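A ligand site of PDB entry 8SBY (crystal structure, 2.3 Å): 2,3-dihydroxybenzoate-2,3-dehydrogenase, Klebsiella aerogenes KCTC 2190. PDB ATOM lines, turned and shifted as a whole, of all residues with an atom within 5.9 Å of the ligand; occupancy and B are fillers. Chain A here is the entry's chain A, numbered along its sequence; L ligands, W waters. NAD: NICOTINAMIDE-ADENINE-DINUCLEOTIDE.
O of Gly 186 sits close to O7N of the ligand (3.3 Å). Gly 23 touches the ligand. Gly 25 touches the ligand. Lys 26 touches the ligand (CE to O2A, 3.4 Å). CA of Gly 27 touches O2N of the ligand, 3.1 Å away. Leu 62 touches the ligand. O of Gly 92 touches C8A of the ligand (3.7 Å). Ile 93 touches the ligand. CG2 of Val 113 touches N6A of the ligand, at 3.7 Å. Val 140 touches the ligand (CG1 to O4D, 3.4 Å). Ala 141 touches the ligand (O to C6N, 3.3 Å). Ser 142 touches the ligand (OG to C5N, 3.2 Å). Pro 185 touches the ligand. CA of Ser 187 touches O7N of the ligand, 3.6 Å away. Hydrophobic or aromatic side chains within 4 Å of the ligand: Ile 28, Leu 48, Val 64, Ala 91, Ile 93, Val 113, Val 140 and Tyr 155. 25 residues have an atom within 4 Å of the ligand: Gly 23, Gly 25, Lys 26, Gly 27, Ile 28, Asp 47, Leu 48, Leu 62, Asp 63, Val 64, Ala 90, Ala 91, Gly 92, Ile 93, Val 113, Val 140, Ala 141, Ser 142, Tyr 155, Lys 159, Pro 185, Gly 186, Ser 187, Thr 188 and Thr 190. The nearest printed residue that does not touch the ligand is Ala 65 (4.2 Å).
The backbone carbonyl oxygen (O) of Phe 46 sits at hydrogen-bond distance from the backbone NH (N) of Gly 23. The backbone carbonyl oxygen (O) of Pro 185 is in hydrogen-bond range of the backbone NH (N) of Asp 143 (2.9 Å). The side-chain hydroxyl of Thr 188 sits at hydrogen-bond distance from the backbone carbonyl oxygen of Gly 186 (2.9 Å). The side-chain carboxylate of Asp 47 lies within hydrogen-bond range of the backbone NH of Gly 25 (2.8 Å). The side-chain hydroxyl of Ser 142 sits at hydrogen-bond distance from the side-chain carboxylate of Asp 143 (3.2 Å). The backbone NH (N) of Ser 142 sits at hydrogen-bond distance from the side-chain hydroxyl (OG) of Ser 184 (3.4 Å). The backbone NH (N) of Ala 91 is in hydrogen-bond range of the side-chain hydroxyl (OG1) of Thr 22 (3.2 Å). The backbone NH (N) of Val 140 sits at hydrogen-bond distance from the backbone carbonyl oxygen (O) of Asn 89 (2.8 Å).
The backbone NH (N) of Leu 48 lies within hydrogen-bond range of a nitrogen (N3A) of the ligand (3.4 Å). O2N of the ligand sits at hydrogen-bond distance from N of Ile 28 (2.6 Å). The side-chain carboxylate of Asp 47 is in hydrogen-bond range of an oxygen (O2B) of the ligand (2.7 Å). An oxygen (O3D) of the ligand is in hydrogen-bond range of the side-chain amino group (NZ) of Lys 159, 2.9 Å away. The side-chain carboxylate (OD1) of Asp 63 lies within hydrogen-bond range of a nitrogen (N6A) of the ligand, 2.9 Å away. O3D of the ligand lies within hydrogen-bond range of O of Ala 91 (3.4 Å). A nitrogen (N1A) of the ligand sits at hydrogen-bond distance from the backbone NH (N) of Val 64. The backbone carbonyl oxygen (O) of Ala 90 lies within hydrogen-bond range of an oxygen (O3D) of the ligand, at 2.8 Å. The side-chain hydroxyl of Thr 190 is in hydrogen-bond range of an oxygen (O1N) of the ligand (3.2 Å). An oxygen (O2D) of the ligand sits at hydrogen-bond distance from the side-chain hydroxyl of Tyr 155, at 2.9 Å. N of Thr 188 is in hydrogen-bond range of O7N of the ligand (2.9 Å).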
ATOM      1  N   THR A  22     -20.437 -14.996  -9.004  1.00  0.00           N
ATOM      2  CA  THR A  22     -21.864 -14.703  -9.096  1.00  0.00           C
ATOM      3  C   THR A  22     -22.351 -14.818 -10.543  1.00  0.00           C
ATOM      4  O   THR A  22     -21.579 -14.648 -11.484  1.00  0.00           O
ATOM      5  CB  THR A  22     -22.173 -13.302  -8.570  1.00  0.00           C
ATOM      6  OG1 THR A  22     -21.528 -12.316  -9.397  1.00  0.00           O
ATOM      7  CG2 THR A  22     -21.685 -13.150  -7.158  1.00  0.00           C
ATOM      8  N   GLY A  23     -23.641 -15.087 -10.709  1.00  0.00           N
ATOM      9  CA  GLY A  23     -24.136 -15.399 -12.051  1.00  0.00           C
ATOM     10  C   GLY A  23     -23.669 -16.739 -12.565  1.00  0.00           C
ATOM     11  O   GLY A  23     -23.701 -16.981 -13.778  1.00  0.00           O
ATOM     12  N   ALA A  24     -23.234 -17.623 -11.678  1.00  0.00           N
ATOM     13  CA  ALA A  24     -22.671 -18.901 -12.066  1.00  0.00           C
ATOM     14  C   ALA A  24     -23.687 -19.831 -12.704  1.00  0.00           C
ATOM     15  O   ALA A  24     -23.297 -20.925 -13.126  1.00  0.00           O
ATOM     16  CB  ALA A  24     -22.032 -19.583 -10.854  1.00  0.00           C
ATOM     17  N   GLY A  25     -24.966 -19.446 -12.779  1.00  0.00           N
ATOM     18  CA  GLY A  25     -25.987 -20.371 -13.245  1.00  0.00           C
ATOM     19  C   GLY A  25     -25.860 -20.713 -14.720  1.00  0.00           C
ATOM     20  O   GLY A  25     -26.136 -21.840 -15.119  1.00  0.00           O
ATOM     21  N   LYS A  26     -25.420 -19.747 -15.539  1.00  0.00           N
ATOM     22  CA  LYS A  26     -25.270 -20.009 -16.960  1.00  0.00           C
ATOM     23  C   LYS A  26     -24.348 -18.955 -17.578  1.00  0.00           C
ATOM     24  O   LYS A  26     -23.742 -18.142 -16.875  1.00  0.00           O
ATOM     25  CB  LYS A  26     -26.637 -20.040 -17.654  1.00  0.00           C
ATOM     26  CG  LYS A  26     -27.424 -18.788 -17.514  1.00  0.00           C
ATOM     27  CD  LYS A  26     -28.817 -18.952 -18.133  1.00  0.00           C
ATOM     28  CE  LYS A  26     -29.460 -17.586 -18.406  1.00  0.00           C
ATOM     29  NZ  LYS A  26     -30.748 -17.684 -19.142  1.00  0.00           N
ATOM     30  N   GLY A  27     -24.219 -19.016 -18.895  1.00  0.00           N
ATOM     31  CA  GLY A  27     -23.456 -18.030 -19.626  1.00  0.00           C
ATOM     32  C   GLY A  27     -22.052 -17.877 -19.096  1.00  0.00           C
ATOM     33  O   GLY A  27     -21.393 -18.836 -18.700  1.00  0.00           O
ATOM     34  N   ILE A  28     -21.590 -16.614 -19.057  1.00  0.00           N
ATOM     35  CA  ILE A  28     -20.203 -16.321 -18.739  1.00  0.00           C
ATOM     36  C   ILE A  28     -19.894 -16.697 -17.303  1.00  0.00           C
ATOM     37  O   ILE A  28     -18.811 -17.221 -16.990  1.00  0.00           O
ATOM     38  CB  ILE A  28     -19.902 -14.841 -19.011  1.00  0.00           C
ATOM     39  CG1 ILE A  28     -19.930 -14.567 -20.512  1.00  0.00           C
ATOM     40  CG2 ILE A  28     -18.565 -14.439 -18.389  1.00  0.00           C
ATOM     41  CD1 ILE A  28     -20.185 -13.112 -20.850  1.00  0.00           C
ATOM     42  N   GLY A  29     -20.838 -16.459 -16.393  1.00  0.00           N
ATOM     43  CA  GLY A  29     -20.630 -16.866 -15.016  1.00  0.00           C
ATOM     44  C   GLY A  29     -20.398 -18.362 -14.879  1.00  0.00           C
ATOM     45  O   GLY A  29     -19.513 -18.804 -14.155  1.00  0.00           O
ATOM     46  N   PHE A  46     -22.868 -18.438  -7.163  1.00  0.00           N
ATOM     47  CA  PHE A  46     -24.039 -17.767  -6.611  1.00  0.00           C
ATOM     48  C   PHE A  46     -24.925 -17.342  -7.759  1.00  0.00           C
ATOM     49  O   PHE A  46     -24.435 -16.839  -8.778  1.00  0.00           O
ATOM     50  CB  PHE A  46     -23.679 -16.514  -5.801  1.00  0.00           C
ATOM     51  CG  PHE A  46     -22.735 -16.780  -4.695  1.00  0.00           C
ATOM     52  CD1 PHE A  46     -21.393 -16.922  -4.938  1.00  0.00           C
ATOM     53  CD2 PHE A  46     -23.200 -16.913  -3.406  1.00  0.00           C
ATOM     54  CE1 PHE A  46     -20.510 -17.176  -3.902  1.00  0.00           C
ATOM     55  CE2 PHE A  46     -22.317 -17.167  -2.370  1.00  0.00           C
ATOM     56  CZ  PHE A  46     -20.964 -17.307  -2.622  1.00  0.00           C
ATOM     57  N   ASP A  47     -26.213 -17.512  -7.583  1.00  0.00           N
ATOM     58  CA  ASP A  47     -27.104 -17.186  -8.679  1.00  0.00           C
ATOM     59  C   ASP A  47     -28.535 -17.196  -8.164  1.00  0.00           C
ATOM     60  O   ASP A  47     -28.856 -17.771  -7.126  1.00  0.00           O
ATOM     61  CB  ASP A  47     -26.938 -18.183  -9.832  1.00  0.00           C
ATOM     62  CG  ASP A  47     -27.412 -17.618 -11.161  1.00  0.00           C
ATOM     63  OD1 ASP A  47     -28.636 -17.475 -11.330  1.00  0.00           O
ATOM     64  OD2 ASP A  47     -26.563 -17.317 -12.028  1.00  0.00           O
ATOM     65  N   LEU A  48     -29.370 -16.510  -8.923  1.00  0.00           N
ATOM     66  CA  LEU A  48     -30.795 -16.482  -8.636  1.00  0.00           C
ATOM     67  C   LEU A  48     -31.369 -17.880  -8.703  1.00  0.00           C
ATOM     68  O   LEU A  48     -32.186 -18.273  -7.871  1.00  0.00           O
ATOM     69  CB  LEU A  48     -31.470 -15.569  -9.669  1.00  0.00           C
ATOM     70  CG  LEU A  48     -32.619 -14.651  -9.328  1.00  0.00           C
ATOM     71  CD1 LEU A  48     -32.474 -14.083  -7.960  1.00  0.00           C
ATOM     72  CD2 LEU A  48     -32.619 -13.541 -10.373  1.00  0.00           C
ATOM     73  N   ALA A  49     -30.902 -18.649  -9.675  1.00  0.00           N
ATOM     74  CA  ALA A  49     -31.467 -19.954  -9.966  1.00  0.00           C
ATOM     75  C   ALA A  49     -30.392 -20.847 -10.532  1.00  0.00           C
ATOM     76  O   ALA A  49     -29.551 -20.409 -11.326  1.00  0.00           O
ATOM     77  CB  ALA A  49     -32.638 -19.865 -10.945  1.00  0.00           C
ATOM     78  N   LEU A  62     -28.918 -17.023  -4.344  1.00  0.00           N
ATOM     79  CA  LEU A  62     -28.644 -15.676  -3.892  1.00  0.00           C
ATOM     80  C   LEU A  62     -29.120 -14.693  -4.939  1.00  0.00           C
ATOM     81  O   LEU A  62     -28.795 -14.840  -6.119  1.00  0.00           O
ATOM     82  CB  LEU A  62     -27.167 -15.489  -3.621  1.00  0.00           C
ATOM     83  CG  LEU A  62     -26.745 -14.095  -3.227  1.00  0.00           C
ATOM     84  CD1 LEU A  62     -27.435 -13.740  -1.895  1.00  0.00           C
ATOM     85  CD2 LEU A  62     -25.203 -13.987  -3.162  1.00  0.00           C
ATOM     86  N   ASP A  63     -29.922 -13.726  -4.510  1.00  0.00           N
ATOM     87  CA  ASP A  63     -30.311 -12.582  -5.323  1.00  0.00           C
ATOM     88  C   ASP A  63     -29.345 -11.465  -4.939  1.00  0.00           C
ATOM     89  O   ASP A  63     -29.485 -10.847  -3.887  1.00  0.00           O
ATOM     90  CB  ASP A  63     -31.773 -12.215  -5.033  1.00  0.00           C
ATOM     91  CG  ASP A  63     -32.211 -10.917  -5.719  1.00  0.00           C
ATOM     92  OD1 ASP A  63     -31.457 -10.306  -6.525  1.00  0.00           O
ATOM     93  OD2 ASP A  63     -33.350 -10.503  -5.435  1.00  0.00           O
ATOM     94  N   VAL A  64     -28.351 -11.223  -5.791  1.00  0.00           N
ATOM     95  CA  VAL A  64     -27.324 -10.259  -5.420  1.00  0.00           C
ATOM     96  C   VAL A  64     -27.909  -8.875  -5.181  1.00  0.00           C
ATOM     97  O   VAL A  64     -27.288  -8.077  -4.473  1.00  0.00           O
ATOM     98  CB  VAL A  64     -26.198 -10.210  -6.475  1.00  0.00           C
ATOM     99  CG1 VAL A  64     -25.477 -11.547  -6.490  1.00  0.00           C
ATOM    100  CG2 VAL A  64     -26.736  -9.855  -7.866  1.00  0.00           C
ATOM    101  N   ALA A  65     -29.092  -8.576  -5.700  1.00  0.00           N
ATOM    102  CA  ALA A  65     -29.649  -7.259  -5.408  1.00  0.00           C
ATOM    103  C   ALA A  65     -30.307  -7.173  -4.038  1.00  0.00           C
ATOM    104  O   ALA A  65     -30.505  -6.072  -3.542  1.00  0.00           O
ATOM    105  CB  ALA A  65     -30.683  -6.829  -6.444  1.00  0.00           C
ATOM    106  N   ASN A  89     -17.529 -10.949  -9.938  1.00  0.00           N
ATOM    107  CA  ASN A  89     -18.862 -10.399 -10.132  1.00  0.00           C
ATOM    108  C   ASN A  89     -19.222 -10.542 -11.601  1.00  0.00           C
ATOM    109  O   ASN A  89     -18.674  -9.834 -12.456  1.00  0.00           O
ATOM    110  CB  ASN A  89     -18.932  -8.923  -9.729  1.00  0.00           C
ATOM    111  CG  ASN A  89     -18.736  -8.695  -8.271  1.00  0.00           C
ATOM    112  OD1 ASN A  89     -19.570  -9.064  -7.454  1.00  0.00           O
ATOM    113  ND2 ASN A  89     -17.655  -8.025  -7.917  1.00  0.00           N
ATOM    114  N   ALA A  90     -20.140 -11.438 -11.896  1.00  0.00           N
ATOM    115  CA  ALA A  90     -20.595 -11.708 -13.248  1.00  0.00           C
ATOM    116  C   ALA A  90     -22.112 -11.713 -13.375  1.00  0.00           C
ATOM    117  O   ALA A  90     -22.607 -11.819 -14.499  1.00  0.00           O
ATOM    118  CB  ALA A  90     -20.051 -13.062 -13.741  1.00  0.00           C
ATOM    119  N   ALA A  91     -22.840 -11.632 -12.287  1.00  0.00           N
ATOM    120  CA  ALA A  91     -24.279 -11.500 -12.370  1.00  0.00           C
ATOM    121  C   ALA A  91     -24.644 -10.219 -13.106  1.00  0.00           C
ATOM    122  O   ALA A  91     -23.927  -9.230 -13.031  1.00  0.00           O
ATOM    123  CB  ALA A  91     -24.881 -11.497 -10.963  1.00  0.00           C
ATOM    124  N   GLY A  92     -25.743 -10.256 -13.827  1.00  0.00           N
ATOM    125  CA  GLY A  92     -26.144  -9.112 -14.620  1.00  0.00           C
ATOM    126  C   GLY A  92     -27.372  -9.439 -15.442  1.00  0.00           C
ATOM    127  O   GLY A  92     -27.623 -10.618 -15.689  1.00  0.00           O
ATOM    128  N   ILE A  93     -28.165  -8.424 -15.831  1.00  0.00           N
ATOM    129  CA  ILE A  93     -29.295  -8.615 -16.719  1.00  0.00           C
ATOM    130  C   ILE A  93     -29.223  -7.554 -17.809  1.00  0.00           C
ATOM    131  O   ILE A  93     -28.598  -6.496 -17.653  1.00  0.00           O
ATOM    132  CB  ILE A  93     -30.666  -8.509 -15.999  1.00  0.00           C
ATOM    133  CG1 ILE A  93     -30.855  -7.096 -15.429  1.00  0.00           C
ATOM    134  CG2 ILE A  93     -30.817  -9.586 -14.916  1.00  0.00           C
ATOM    135  CD1 ILE A  93     -32.192  -6.857 -14.742  1.00  0.00           C
ATOM    136  N   LEU A  94     -29.923  -7.846 -18.905  1.00  0.00           N
ATOM    137  CA  LEU A  94     -30.045  -6.950 -20.050  1.00  0.00           C
ATOM    138  C   LEU A  94     -31.522  -6.637 -20.252  1.00  0.00           C
ATOM    139  O   LEU A  94     -32.326  -7.548 -20.470  1.00  0.00           O
ATOM    140  CB  LEU A  94     -29.425  -7.600 -21.302  1.00  0.00           C
ATOM    141  CG  LEU A  94     -29.621  -6.885 -22.636  1.00  0.00           C
ATOM    142  CD1 LEU A  94     -28.974  -5.497 -22.640  1.00  0.00           C
ATOM    143  CD2 LEU A  94     -29.080  -7.696 -23.816  1.00  0.00           C
ATOM    144  N   VAL A 113     -29.588  -4.746 -10.015  1.00  0.00           N
ATOM    145  CA  VAL A 113     -28.812  -5.967 -10.262  1.00  0.00           C
ATOM    146  C   VAL A 113     -27.393  -5.636 -10.737  1.00  0.00           C
ATOM    147  O   VAL A 113     -26.413  -6.131 -10.187  1.00  0.00           O
ATOM    148  CB  VAL A 113     -29.532  -6.868 -11.283  1.00  0.00           C
ATOM    149  CG1 VAL A 113     -28.696  -8.068 -11.585  1.00  0.00           C
ATOM    150  CG2 VAL A 113     -30.917  -7.285 -10.751  1.00  0.00           C
ATOM    151  N   ASN A 114     -27.267  -4.790 -11.763  1.00  0.00           N
ATOM    152  CA  ASN A 114     -25.985  -4.665 -12.453  1.00  0.00           C
ATOM    153  C   ASN A 114     -24.968  -3.844 -11.649  1.00  0.00           C
ATOM    154  O   ASN A 114     -23.755  -4.020 -11.852  1.00  0.00           O
ATOM    155  CB  ASN A 114     -26.201  -4.037 -13.828  1.00  0.00           C
ATOM    156  CG  ASN A 114     -26.873  -4.968 -14.799  1.00  0.00           C
ATOM    157  OD1 ASN A 114     -27.176  -6.100 -14.470  1.00  0.00           O
ATOM    158  ND2 ASN A 114     -27.122  -4.481 -15.999  1.00  0.00           N
ATOM    159  N   VAL A 140     -17.224  -8.361 -14.352  1.00  0.00           N
ATOM    160  CA  VAL A 140     -17.587  -8.346 -15.759  1.00  0.00           C
ATOM    161  C   VAL A 140     -18.482  -7.143 -16.033  1.00  0.00           C
ATOM    162  O   VAL A 140     -19.632  -7.070 -15.545  1.00  0.00           O
ATOM    163  CB  VAL A 140     -18.292  -9.647 -16.149  1.00  0.00           C
ATOM    164  CG1 VAL A 140     -18.681  -9.599 -17.625  1.00  0.00           C
ATOM    165  CG2 VAL A 140     -17.411 -10.848 -15.837  1.00  0.00           C
ATOM    166  N   ALA A 141     -17.964  -6.200 -16.819  1.00  0.00           N
ATOM    167  CA  ALA A 141     -18.743  -5.071 -17.313  1.00  0.00           C
ATOM    168  C   ALA A 141     -19.362  -5.383 -18.680  1.00  0.00           C
ATOM    169  O   ALA A 141     -20.184  -6.295 -18.799  1.00  0.00           O
ATOM    170  CB  ALA A 141     -17.865  -3.825 -17.392  1.00  0.00           C
ATOM    171  N   SER A 142     -18.977  -4.617 -19.705  1.00  0.00           N
ATOM    172  CA  SER A 142     -19.538  -4.790 -21.042  1.00  0.00           C
ATOM    173  C   SER A 142     -18.912  -3.777 -21.997  1.00  0.00           C
ATOM    174  O   SER A 142     -18.480  -2.715 -21.580  1.00  0.00           O
ATOM    175  CB  SER A 142     -21.043  -4.570 -21.053  1.00  0.00           C
ATOM    176  OG  SER A 142     -21.522  -4.641 -22.373  1.00  0.00           O
ATOM    177  N   ASP A 143     -18.917  -4.112 -23.306  1.00  0.00           N
ATOM    178  CA  ASP A 143     -18.438  -3.128 -24.285  1.00  0.00           C
ATOM    179  C   ASP A 143     -19.339  -1.913 -24.287  1.00  0.00           C
ATOM    180  O   ASP A 143     -18.911  -0.839 -24.746  1.00  0.00           O
ATOM    181  CB  ASP A 143     -18.348  -3.726 -25.701  1.00  0.00           C
ATOM    182  CG  ASP A 143     -19.691  -4.224 -26.251  1.00  0.00           C
ATOM    183  OD1 ASP A 143     -20.599  -4.587 -25.455  1.00  0.00           O
ATOM    184  OD2 ASP A 143     -19.817  -4.236 -27.494  1.00  0.00           O
ATOM    185  N   TYR A 155     -28.681  -0.148 -19.889  1.00  0.00           N
ATOM    186  CA  TYR A 155     -27.749  -1.223 -19.678  1.00  0.00           C
ATOM    187  C   TYR A 155     -26.322  -0.701 -19.720  1.00  0.00           C
ATOM    188  O   TYR A 155     -25.512  -0.990 -18.821  1.00  0.00           O
ATOM    189  CB  TYR A 155     -27.988  -2.298 -20.729  1.00  0.00           C
ATOM    190  CG  TYR A 155     -27.007  -3.422 -20.648  1.00  0.00           C
ATOM    191  CD1 TYR A 155     -27.134  -4.415 -19.685  1.00  0.00           C
ATOM    192  CD2 TYR A 155     -25.954  -3.484 -21.536  1.00  0.00           C
ATOM    193  CE1 TYR A 155     -26.183  -5.476 -19.616  1.00  0.00           C
ATOM    194  CE2 TYR A 155     -25.045  -4.508 -21.486  1.00  0.00           C
ATOM    195  CZ  TYR A 155     -25.151  -5.497 -20.531  1.00  0.00           C
ATOM    196  OH  TYR A 155     -24.197  -6.484 -20.542  1.00  0.00           O
ATOM    197  N   LYS A 159     -23.527  -0.505 -16.545  1.00  0.00           N
ATOM    198  CA  LYS A 159     -22.229  -1.147 -16.587  1.00  0.00           C
ATOM    199  C   LYS A 159     -21.087  -0.141 -16.492  1.00  0.00           C
ATOM    200  O   LYS A 159     -19.978  -0.485 -16.046  1.00  0.00           O
ATOM    201  CB  LYS A 159     -22.102  -1.956 -17.870  1.00  0.00           C
ATOM    202  CG  LYS A 159     -23.030  -3.183 -17.901  1.00  0.00           C
ATOM    203  CD  LYS A 159     -22.601  -4.241 -16.901  1.00  0.00           C
ATOM    204  CE  LYS A 159     -23.136  -5.608 -17.302  1.00  0.00           C
ATOM    205  NZ  LYS A 159     -22.411  -6.694 -16.577  1.00  0.00           N
ATOM    206  N   SER A 184     -14.571  -6.639 -20.152  1.00  0.00           N
ATOM    207  CA  SER A 184     -15.720  -6.022 -20.799  1.00  0.00           C
ATOM    208  C   SER A 184     -16.001  -6.778 -22.089  1.00  0.00           C
ATOM    209  O   SER A 184     -15.376  -6.521 -23.120  1.00  0.00           O
ATOM    210  CB  SER A 184     -15.450  -4.548 -21.054  1.00  0.00           C
ATOM    211  OG  SER A 184     -15.628  -3.852 -19.844  1.00  0.00           O
ATOM    212  N   PRO A 185     -16.884  -7.775 -22.031  1.00  0.00           N
ATOM    213  CA  PRO A 185     -17.161  -8.560 -23.246  1.00  0.00           C
ATOM    214  C   PRO A 185     -17.963  -7.780 -24.266  1.00  0.00           C
ATOM    215  O   PRO A 185     -18.848  -6.992 -23.928  1.00  0.00           O
ATOM    216  CB  PRO A 185     -17.981  -9.744 -22.710  1.00  0.00           C
ATOM    217  CG  PRO A 185     -17.781  -9.778 -21.299  1.00  0.00           C
ATOM    218  CD  PRO A 185     -17.383  -8.430 -20.822  1.00  0.00           C
ATOM    219  N   GLY A 186     -17.638  -8.004 -25.528  1.00  0.00           N
ATOM    220  CA  GLY A 186     -18.545  -7.725 -26.621  1.00  0.00           C
ATOM    221  C   GLY A 186     -19.499  -8.892 -26.824  1.00  0.00           C
ATOM    222  O   GLY A 186     -19.706  -9.720 -25.923  1.00  0.00           O
ATOM    223  N   SER A 187     -20.068  -8.981 -28.021  1.00  0.00           N
ATOM    224  CA  SER A 187     -21.067  -9.986 -28.312  1.00  0.00           C
ATOM    225  C   SER A 187     -20.473 -11.367 -28.033  1.00  0.00           C
ATOM    226  O   SER A 187     -19.397 -11.697 -28.528  1.00  0.00           O
ATOM    227  CB  SER A 187     -21.520  -9.911 -29.759  1.00  0.00           C
ATOM    228  OG  SER A 187     -22.185  -8.694 -30.066  1.00  0.00           O
ATOM    229  N   THR A 188     -21.173 -12.148 -27.208  1.00  0.00           N
ATOM    230  CA  THR A 188     -20.796 -13.486 -26.779  1.00  0.00           C
ATOM    231  C   THR A 188     -21.963 -14.435 -27.047  1.00  0.00           C
ATOM    232  O   THR A 188     -23.123 -14.024 -26.999  1.00  0.00           O
ATOM    233  CB  THR A 188     -20.428 -13.513 -25.257  1.00  0.00           C
ATOM    234  OG1 THR A 188     -19.519 -12.459 -24.953  1.00  0.00           O
ATOM    235  CG2 THR A 188     -19.793 -14.801 -24.812  1.00  0.00           C
ATOM    236  N   ASP A 189     -21.648 -15.696 -27.315  1.00  0.00           N
ATOM    237  CA  ASP A 189     -22.659 -16.733 -27.583  1.00  0.00           C
ATOM    238  C   ASP A 189     -23.285 -17.252 -26.275  1.00  0.00           C
ATOM    239  O   ASP A 189     -22.816 -18.228 -25.687  1.00  0.00           O
ATOM    240  CB  ASP A 189     -22.021 -17.883 -28.364  1.00  0.00           C
ATOM    241  CG  ASP A 189     -23.021 -18.650 -29.203  1.00  0.00           C
ATOM    242  OD1 ASP A 189     -24.102 -19.027 -28.680  1.00  0.00           O
ATOM    243  OD2 ASP A 189     -22.735 -18.867 -30.410  1.00  0.00           O
ATOM    244  N   THR A 190     -24.365 -16.603 -25.831  1.00  0.00           N
ATOM    245  CA  THR A 190     -25.207 -17.085 -24.726  1.00  0.00           C
ATOM    246  C   THR A 190     -26.679 -16.995 -25.133  1.00  0.00           C
ATOM    247  O   THR A 190     -27.255 -15.903 -25.140  1.00  0.00           O
ATOM    248  CB  THR A 190     -25.017 -16.288 -23.402  1.00  0.00           C
ATOM    249  OG1 THR A 190     -25.600 -14.976 -23.539  1.00  0.00           O
ATOM    250  CG2 THR A 190     -23.541 -16.164 -22.991  1.00  0.00           C
HETATM  251  PA  NAD L   1     -27.024 -14.894 -18.892  1.00  0.00           P
HETATM  252  O1A NAD L   1     -28.351 -14.216 -18.767  1.00  0.00           O
HETATM  253  O2A NAD L   1     -26.804 -16.056 -19.794  1.00  0.00           O
HETATM  254  O5B NAD L   1     -26.502 -15.323 -17.402  1.00  0.00           O
HETATM  255  C5B NAD L   1     -26.347 -14.374 -16.376  1.00  0.00           C
HETATM  256  C4B NAD L   1     -26.678 -14.996 -15.028  1.00  0.00           C
HETATM  257  O4B NAD L   1     -26.845 -13.907 -14.090  1.00  0.00           O
HETATM  258  C3B NAD L   1     -27.974 -15.819 -15.003  1.00  0.00           C
HETATM  259  O3B NAD L   1     -27.707 -17.094 -14.493  1.00  0.00           O
HETATM  260  C2B NAD L   1     -28.830 -15.061 -13.996  1.00  0.00           C
HETATM  261  O2B NAD L   1     -29.652 -15.877 -13.223  1.00  0.00           O
HETATM  262  C1B NAD L   1     -27.772 -14.315 -13.147  1.00  0.00           C
HETATM  263  N9A NAD L   1     -28.460 -13.294 -12.407  1.00  0.00           N
HETATM  264  C8A NAD L   1     -29.329 -12.367 -12.927  1.00  0.00           C
HETATM  265  N7A NAD L   1     -29.863 -11.601 -12.034  1.00  0.00           N
HETATM  266  C5A NAD L   1     -29.330 -12.022 -10.838  1.00  0.00           C
HETATM  267  C6A NAD L   1     -29.497 -11.588  -9.502  1.00  0.00           C
HETATM  268  N6A NAD L   1     -30.307 -10.575  -9.162  1.00  0.00           N
HETATM  269  N1A NAD L   1     -28.828 -12.238  -8.534  1.00  0.00           N
HETATM  270  C2A NAD L   1     -28.042 -13.245  -8.858  1.00  0.00           C
HETATM  271  N3A NAD L   1     -27.791 -13.739 -10.074  1.00  0.00           N
HETATM  272  C4A NAD L   1     -28.461 -13.088 -11.032  1.00  0.00           C
HETATM  273  O3  NAD L   1     -25.920 -13.701 -19.201  1.00  0.00           O
HETATM  274  PN  NAD L   1     -24.369 -13.800 -19.707  1.00  0.00           P
HETATM  275  O1N NAD L   1     -24.327 -13.368 -21.148  1.00  0.00           O
HETATM  276  O2N NAD L   1     -23.635 -14.985 -19.212  1.00  0.00           O
HETATM  277  O5D NAD L   1     -23.839 -12.530 -18.858  1.00  0.00           O
HETATM  278  C5D NAD L   1     -22.863 -12.707 -17.851  1.00  0.00           C
HETATM  279  C4D NAD L   1     -22.195 -11.374 -17.653  1.00  0.00           C
HETATM  280  O4D NAD L   1     -21.609 -10.854 -18.875  1.00  0.00           O
HETATM  281  C3D NAD L   1     -23.254 -10.369 -17.211  1.00  0.00           C
HETATM  282  O3D NAD L   1     -22.692  -9.562 -16.207  1.00  0.00           O
HETATM  283  C2D NAD L   1     -23.548  -9.643 -18.548  1.00  0.00           C
HETATM  284  O2D NAD L   1     -24.148  -8.390 -18.374  1.00  0.00           O
HETATM  285  C1D NAD L   1     -22.143  -9.611 -19.200  1.00  0.00           C
HETATM  286  N1N NAD L   1     -22.128  -9.344 -20.695  1.00  0.00           N
HETATM  287  C2N NAD L   1     -22.548 -10.251 -21.607  1.00  0.00           C
HETATM  288  C3N NAD L   1     -22.523  -9.949 -22.972  1.00  0.00           C
HETATM  289  C7N NAD L   1     -22.982 -10.926 -24.043  1.00  0.00           C
HETATM  290  O7N NAD L   1     -22.747 -10.667 -25.225  1.00  0.00           O
HETATM  291  N7N NAD L   1     -23.623 -12.018 -23.608  1.00  0.00           N
HETATM  292  C4N NAD L   1     -22.057  -8.708 -23.397  1.00  0.00           C
HETATM  293  C5N NAD L   1     -21.621  -7.791 -22.454  1.00  0.00           C
HETATM  294  C6N NAD L   1     -21.672  -8.137 -21.116  1.00  0.00           C
HETATM  295  O   HOH W   1     -20.964  -8.454 -13.524  1.00  0.00           O
